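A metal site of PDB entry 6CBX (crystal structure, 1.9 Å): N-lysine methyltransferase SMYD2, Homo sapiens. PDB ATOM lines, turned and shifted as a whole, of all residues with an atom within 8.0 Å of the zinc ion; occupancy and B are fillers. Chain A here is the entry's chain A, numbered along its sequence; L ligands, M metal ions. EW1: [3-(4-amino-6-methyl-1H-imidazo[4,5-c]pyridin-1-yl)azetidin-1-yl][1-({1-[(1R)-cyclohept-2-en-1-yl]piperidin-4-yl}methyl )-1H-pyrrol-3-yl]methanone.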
ATOM      1  N   HIS A 208      34.816 -22.501   2.147  1.00  0.00           N
ATOM      2  CA  HIS A 208      33.885 -23.505   2.602  1.00  0.00           C
ATOM      3  C   HIS A 208      32.958 -23.972   1.489  1.00  0.00           C
ATOM      4  O   HIS A 208      32.463 -23.145   0.710  1.00  0.00           O
ATOM      5  CB  HIS A 208      33.016 -22.977   3.751  1.00  0.00           C
ATOM      6  CG  HIS A 208      31.826 -23.837   4.018  1.00  0.00           C
ATOM      7  ND1 HIS A 208      31.901 -24.948   4.815  1.00  0.00           N
ATOM      8  CD2 HIS A 208      30.585 -23.843   3.475  1.00  0.00           C
ATOM      9  CE1 HIS A 208      30.731 -25.570   4.820  1.00  0.00           C
ATOM     10  NE2 HIS A 208      29.925 -24.930   3.988  1.00  0.00           N
ATOM     11  N   SER A 209      32.705 -25.282   1.438  1.00  0.00           N
ATOM     12  CA  SER A 209      31.571 -25.889   0.756  1.00  0.00           C
ATOM     13  C   SER A 209      31.006 -27.041   1.613  1.00  0.00           C
ATOM     14  O   SER A 209      31.738 -27.692   2.371  1.00  0.00           O
ATOM     15  CB  SER A 209      31.983 -26.419  -0.635  1.00  0.00           C
ATOM     16  OG  SER A 209      30.941 -27.126  -1.260  1.00  0.00           O
ATOM     17  N   CYS A 210      29.701 -27.298   1.483  1.00  0.00           N
ATOM     18  CA  CYS A 210      29.093 -28.505   2.079  1.00  0.00           C
ATOM     19  C   CYS A 210      29.309 -29.803   1.274  1.00  0.00           C
ATOM     20  O   CYS A 210      28.967 -30.890   1.773  1.00  0.00           O
ATOM     21  CB  CYS A 210      27.610 -28.301   2.353  1.00  0.00           C
ATOM     22  SG  CYS A 210      27.229 -26.750   3.223  1.00  0.00           S
ATOM     23  N   CYS A 211      29.847 -29.708   0.055  1.00  0.00           N
ATOM     24  CA  CYS A 211      30.446 -30.849  -0.645  1.00  0.00           C
ATOM     25  C   CYS A 211      31.924 -30.533  -0.874  1.00  0.00           C
ATOM     26  O   CYS A 211      32.364 -30.221  -1.986  1.00  0.00           O
ATOM     27  CB  CYS A 211      29.721 -31.159  -1.958  1.00  0.00           C
ATOM     28  SG  CYS A 211      28.999 -29.724  -2.740  1.00  0.00           S
ATOM     29  N   SER A 240      35.301 -28.067   4.553  1.00  0.00           N
ATOM     30  CA  SER A 240      34.086 -27.740   5.297  1.00  0.00           C
ATOM     31  C   SER A 240      34.428 -27.132   6.657  1.00  0.00           C
ATOM     32  O   SER A 240      35.285 -27.640   7.356  1.00  0.00           O
ATOM     33  CB  SER A 240      33.166 -28.962   5.512  1.00  0.00           C
ATOM     34  OG  SER A 240      32.063 -28.550   6.327  1.00  0.00           O
ATOM     35  N   ILE A 242      31.939 -26.725   8.878  1.00  0.00           N
ATOM     36  CA  ILE A 242      30.856 -27.141   9.777  1.00  0.00           C
ATOM     37  C   ILE A 242      30.618 -28.647   9.678  1.00  0.00           C
ATOM     38  O   ILE A 242      31.188 -29.327   8.834  1.00  0.00           O
ATOM     39  CB  ILE A 242      29.545 -26.315   9.595  1.00  0.00           C
ATOM     40  CG1 ILE A 242      29.104 -26.148   8.117  1.00  0.00           C
ATOM     41  CG2 ILE A 242      29.699 -24.935  10.220  1.00  0.00           C
ATOM     42  CD1 ILE A 242      28.471 -27.380   7.502  1.00  0.00           C
ATOM     43  N   LEU A 244      28.719 -31.713   8.638  1.00  0.00           N
ATOM     44  CA  LEU A 244      27.919 -31.945   7.468  1.00  0.00           C
ATOM     45  C   LEU A 244      26.729 -32.903   7.700  1.00  0.00           C
ATOM     46  O   LEU A 244      25.964 -33.152   6.762  1.00  0.00           O
ATOM     47  CB  LEU A 244      28.816 -32.449   6.345  1.00  0.00           C
ATOM     48  CG  LEU A 244      29.926 -31.458   5.916  1.00  0.00           C
ATOM     49  CD1 LEU A 244      30.924 -32.117   4.959  1.00  0.00           C
ATOM     50  CD2 LEU A 244      29.317 -30.218   5.291  1.00  0.00           C
ATOM     51  N   THR A 248      20.298 -28.220   5.592  1.00  0.00           N
ATOM     52  CA  THR A 248      20.735 -26.946   5.066  1.00  0.00           C
ATOM     53  C   THR A 248      20.572 -25.795   6.072  1.00  0.00           C
ATOM     54  O   THR A 248      21.531 -25.056   6.314  1.00  0.00           O
ATOM     55  CB  THR A 248      20.076 -26.680   3.687  1.00  0.00           C
ATOM     56  OG1 THR A 248      20.459 -27.722   2.788  1.00  0.00           O
ATOM     57  CG2 THR A 248      20.509 -25.357   3.111  1.00  0.00           C
ATOM     58  N   ARG A 251      23.091 -26.078   8.989  1.00  0.00           N
ATOM     59  CA  ARG A 251      24.450 -25.832   8.498  1.00  0.00           C
ATOM     60  C   ARG A 251      24.711 -24.314   8.394  1.00  0.00           C
ATOM     61  O   ARG A 251      25.691 -23.779   8.905  1.00  0.00           O
ATOM     62  CB  ARG A 251      24.639 -26.518   7.153  1.00  0.00           C
ATOM     63  CG  ARG A 251      24.750 -28.024   7.265  1.00  0.00           C
ATOM     64  CD  ARG A 251      25.318 -28.665   6.019  1.00  0.00           C
ATOM     65  NE  ARG A 251      24.788 -28.179   4.735  1.00  0.00           N
ATOM     66  CZ  ARG A 251      23.713 -28.666   4.103  1.00  0.00           C
ATOM     67  NH1 ARG A 251      22.968 -29.638   4.624  1.00  0.00           N
ATOM     68  NH2 ARG A 251      23.353 -28.148   2.926  1.00  0.00           N
ATOM     69  N   ASN A 252      23.766 -23.639   7.737  1.00  0.00           N
ATOM     70  CA  ASN A 252      23.852 -22.209   7.532  1.00  0.00           C
ATOM     71  C   ASN A 252      23.698 -21.370   8.790  1.00  0.00           C
ATOM     72  O   ASN A 252      24.320 -20.305   8.900  1.00  0.00           O
ATOM     73  CB  ASN A 252      22.916 -21.800   6.397  1.00  0.00           C
ATOM     74  CG  ASN A 252      23.504 -22.160   5.056  1.00  0.00           C
ATOM     75  OD1 ASN A 252      24.341 -21.430   4.545  1.00  0.00           O
ATOM     76  ND2 ASN A 252      23.099 -23.300   4.502  1.00  0.00           N
ATOM     77  N   LEU A 255      27.146 -21.597  10.176  1.00  0.00           N
ATOM     78  CA  LEU A 255      28.072 -20.722   9.442  1.00  0.00           C
ATOM     79  C   LEU A 255      27.866 -19.274   9.842  1.00  0.00           C
ATOM     80  O   LEU A 255      28.821 -18.545  10.092  1.00  0.00           O
ATOM     81  CB  LEU A 255      27.880 -20.899   7.939  1.00  0.00           C
ATOM     82  CG  LEU A 255      28.378 -22.232   7.399  1.00  0.00           C
ATOM     83  CD1 LEU A 255      27.839 -22.380   6.000  1.00  0.00           C
ATOM     84  CD2 LEU A 255      29.907 -22.302   7.436  1.00  0.00           C
ATOM     85  N   PHE A 261      28.446 -15.633   7.311  1.00  0.00           N
ATOM     86  CA  PHE A 261      28.095 -15.816   5.911  1.00  0.00           C
ATOM     87  C   PHE A 261      27.217 -17.036   5.776  1.00  0.00           C
ATOM     88  O   PHE A 261      27.119 -17.853   6.678  1.00  0.00           O
ATOM     89  CB  PHE A 261      29.349 -15.940   5.011  1.00  0.00           C
ATOM     90  CG  PHE A 261      30.055 -17.279   5.085  1.00  0.00           C
ATOM     91  CD1 PHE A 261      31.065 -17.494   6.019  1.00  0.00           C
ATOM     92  CD2 PHE A 261      29.722 -18.322   4.204  1.00  0.00           C
ATOM     93  CE1 PHE A 261      31.761 -18.714   6.060  1.00  0.00           C
ATOM     94  CE2 PHE A 261      30.396 -19.546   4.266  1.00  0.00           C
ATOM     95  CZ  PHE A 261      31.411 -19.727   5.188  1.00  0.00           C
ATOM     96  N   THR A 262      26.551 -17.126   4.629  1.00  0.00           N
ATOM     97  CA  THR A 262      25.707 -18.267   4.277  1.00  0.00           C
ATOM     98  C   THR A 262      26.288 -18.928   3.036  1.00  0.00           C
ATOM     99  O   THR A 262      26.892 -18.269   2.192  1.00  0.00           O
ATOM    100  CB  THR A 262      24.261 -17.826   4.011  1.00  0.00           C
ATOM    101  OG1 THR A 262      24.256 -16.814   3.024  1.00  0.00           O
ATOM    102  CG2 THR A 262      23.624 -17.255   5.271  1.00  0.00           C
ATOM    103  N   CYS A 263      26.092 -20.243   2.921  1.00  0.00           N
ATOM    104  CA  CYS A 263      26.708 -21.038   1.863  1.00  0.00           C
ATOM    105  C   CYS A 263      25.855 -21.020   0.601  1.00  0.00           C
ATOM    106  O   CYS A 263      24.651 -20.924   0.670  1.00  0.00           O
ATOM    107  CB  CYS A 263      26.913 -22.478   2.310  1.00  0.00           C
ATOM    108  SG  CYS A 263      27.883 -23.452   1.122  1.00  0.00           S
ATOM    109  N   GLU A 264      26.517 -21.164  -0.544  1.00  0.00           N
ATOM    110  CA  GLU A 264      25.887 -21.162  -1.865  1.00  0.00           C
ATOM    111  C   GLU A 264      26.207 -22.414  -2.671  1.00  0.00           C
ATOM    112  O   GLU A 264      25.868 -22.479  -3.857  1.00  0.00           O
ATOM    113  CB  GLU A 264      26.274 -19.890  -2.658  1.00  0.00           C
ATOM    114  CG  GLU A 264      27.774 -19.690  -2.947  1.00  0.00           C
ATOM    115  CD  GLU A 264      28.623 -19.520  -1.679  1.00  0.00           C
ATOM    116  OE1 GLU A 264      29.165 -20.528  -1.182  1.00  0.00           O
ATOM    117  OE2 GLU A 264      28.678 -18.420  -1.121  1.00  0.00           O
ATOM    118  N   CYS A 265      26.787 -23.431  -2.032  1.00  0.00           N
ATOM    119  CA  CYS A 265      27.114 -24.673  -2.743  1.00  0.00           C
ATOM    120  C   CYS A 265      25.880 -25.417  -3.302  1.00  0.00           C
ATOM    121  O   CYS A 265      24.738 -25.070  -3.007  1.00  0.00           O
ATOM    122  CB  CYS A 265      27.916 -25.620  -1.842  1.00  0.00           C
ATOM    123  SG  CYS A 265      26.962 -26.544  -0.636  1.00  0.00           S
ATOM    124  N   GLN A 266      26.122 -26.455  -4.085  1.00  0.00           N
ATOM    125  CA  GLN A 266      25.039 -27.222  -4.703  1.00  0.00           C
ATOM    126  C   GLN A 266      24.105 -27.829  -3.647  1.00  0.00           C
ATOM    127  O   GLN A 266      22.887 -27.765  -3.802  1.00  0.00           O
ATOM    128  CB  GLN A 266      25.580 -28.316  -5.659  1.00  0.00           C
ATOM    129  CG  GLN A 266      24.597 -28.725  -6.736  1.00  0.00           C
ATOM    130  N   GLU A 267      24.665 -28.357  -2.558  1.00  0.00           N
ATOM    131  CA  GLU A 267      23.839 -28.957  -1.490  1.00  0.00           C
ATOM    132  C   GLU A 267      22.872 -27.930  -0.876  1.00  0.00           C
ATOM    133  O   GLU A 267      21.713 -28.254  -0.622  1.00  0.00           O
ATOM    134  CB  GLU A 267      24.692 -29.562  -0.373  1.00  0.00           C
ATOM    135  CG  GLU A 267      25.614 -30.699  -0.817  1.00  0.00           C
ATOM    136  CD  GLU A 267      24.881 -31.995  -1.169  1.00  0.00           C
ATOM    137  OE1 GLU A 267      23.633 -32.058  -1.066  1.00  0.00           O
ATOM    138  OE2 GLU A 267      25.590 -32.971  -1.541  1.00  0.00           O
ATOM    139  N   CYS A 268      23.358 -26.718  -0.666  1.00  0.00           N
ATOM    140  CA  CYS A 268      22.567 -25.661  -0.047  1.00  0.00           C
ATOM    141  C   CYS A 268      21.544 -25.015  -0.988  1.00  0.00           C
ATOM    142  O   CYS A 268      20.488 -24.586  -0.551  1.00  0.00           O
ATOM    143  CB  CYS A 268      23.485 -24.589   0.514  1.00  0.00           C
ATOM    144  SG  CYS A 268      24.405 -25.135   1.965  1.00  0.00           S
ATOM    145  N   THR A 269      21.912 -24.881  -2.267  1.00  0.00           N
ATOM    146  CA  THR A 269      21.041 -24.331  -3.306  1.00  0.00           C
ATOM    147  C   THR A 269      19.826 -25.235  -3.534  1.00  0.00           C
ATOM    148  O   THR A 269      18.678 -24.803  -3.435  1.00  0.00           O
ATOM    149  CB  THR A 269      21.851 -24.188  -4.630  1.00  0.00           C
ATOM    150  OG1 THR A 269      22.814 -23.137  -4.476  1.00  0.00           O
ATOM    151  CG2 THR A 269      20.965 -23.857  -5.846  1.00  0.00           C
HETATM  152  C4  EW1 L   1      32.643 -19.023   1.855  1.00  0.00           C
HETATM  153  C5  EW1 L   1      34.484 -19.075   2.901  1.00  0.00           C
HETATM  154  C6  EW1 L   1      34.828 -16.628   3.467  1.00  0.00           C
HETATM  155  N1  EW1 L   1      34.105 -17.764   2.909  1.00  0.00           N
HETATM  156  C7  EW1 L   1      35.968 -17.000   4.454  1.00  0.00           C
HETATM  157  C8  EW1 L   1      34.056 -16.010   4.648  1.00  0.00           C
HETATM  158  N2  EW1 L   1      35.143 -16.434   5.540  1.00  0.00           N
HETATM  159  C9  EW1 L   1      35.167 -16.224   6.858  1.00  0.00           C
HETATM  160  C10 EW1 L   1      36.256 -16.834   7.642  1.00  0.00           C
HETATM  161  C11 EW1 L   1      37.037 -17.909   7.266  1.00  0.00           C
HETATM  162  C12 EW1 L   1      38.875 -19.296   8.272  1.00  0.00           C
HETATM  163  N3  EW1 L   1      37.935 -18.180   8.259  1.00  0.00           N
HETATM  164  C13 EW1 L   1      38.564 -20.302   9.337  1.00  0.00           C
HETATM  165  C14 EW1 L   1      37.303 -21.073   9.008  1.00  0.00           C
HETATM  166  C15 EW1 L   1      36.966 -22.070  10.095  1.00  0.00           C
HETATM  167  N4  EW1 L   1      38.091 -23.006  10.346  1.00  0.00           N
HETATM  168  O   EW1 L   1      34.393 -15.437   7.391  1.00  0.00           O
HETATM  169  C3  EW1 L   1      32.898 -17.714   2.245  1.00  0.00           C
HETATM  170  C2  EW1 L   1      32.061 -16.660   1.907  1.00  0.00           C
HETATM  171  N   EW1 L   1      33.645 -19.874   2.282  1.00  0.00           N
HETATM  172  C27 EW1 L   1      31.475 -19.272   1.128  1.00  0.00           C
HETATM  173  N5  EW1 L   1      31.142 -20.482   0.700  1.00  0.00           N
HETATM  174  N6  EW1 L   1      30.624 -18.258   0.841  1.00  0.00           N
HETATM  175  C1  EW1 L   1      30.878 -17.000   1.251  1.00  0.00           C
HETATM  176  C   EW1 L   1      29.796 -15.981   0.999  1.00  0.00           C
HETATM  177  C26 EW1 L   1      36.711 -16.430   8.952  1.00  0.00           C
HETATM  178  C25 EW1 L   1      37.724 -17.275   9.277  1.00  0.00           C
HETATM  179  C17 EW1 L   1      39.684 -21.293   9.584  1.00  0.00           C
HETATM  180  C16 EW1 L   1      39.313 -22.251  10.692  1.00  0.00           C
HETATM  181  C18 EW1 L   1      37.802 -24.189  11.171  1.00  0.00           C
HETATM  182  C24 EW1 L   1      37.437 -23.716  12.548  1.00  0.00           C
HETATM  183  C23 EW1 L   1      37.214 -24.491  13.617  1.00  0.00           C
HETATM  184  C22 EW1 L   1      37.230 -25.984  13.651  1.00  0.00           C
HETATM  185  C21 EW1 L   1      36.241 -26.651  12.686  1.00  0.00           C
HETATM  186  C20 EW1 L   1      36.762 -26.555  11.261  1.00  0.00           C
HETATM  187  C19 EW1 L   1      36.736 -25.161  10.636  1.00  0.00           C
HETATM  188 ZN    ZN M   1      26.649 -25.414   1.396  1.00  0.00          ZN
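The side-chain sulfur (SG) of Cys 268 lies close to the guanidinium group (NH2) of Arg 251. The backbone NH (N) of Cys 263 sits at hydrogen-bond distance from the side-chain amide oxygen (OD1) of Asn 252, at 2.7 Å. N of Cys 210 is in hydrogen-bond range of NE2 of His 208 (3.5 Å). The side-chain sulfur (SG) of Cys 268 sits close to the side-chain amide nitrogen (ND2) of Asn 252 (3.4 Å). The guanidinium group of Arg 251 sits close to the side-chain sulfur of Cys 210, at 3.2 Å. The side-chain sulfur (SG) of Cys 265 sits close to the backbone NH (N) of Glu 267 (3.5 Å). The side-chain hydroxyl (OG1) of Thr 269 lies within hydrogen-bond range of the backbone carbonyl oxygen (O) of Cys 265 (3.1 Å).
The zinc ion is bound by SG of Cys 268 (2.3 Å), SG of Cys 263 (2.3 Å), SG of Cys 210 (2.3 Å) and SG of Cys 265 (2.3 Å). The zinc ion has four donor atoms within binding distance.
The backbone carbonyl oxygen of His 208 is in hydrogen-bond range of a nitrogen (N5) of the ligand (3.0 Å). N5 of the ligand lies within hydrogen-bond range of OE1 of Glu 264 (2.7 Å). N of His 208 is in hydrogen-bond range of N of the ligand (2.9 Å).
Of the 20 residues printed, 4 come within 4 Å of the zinc ion. The nearest printed residue that does not touch the zinc ion is His 208 (4.2 Å).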
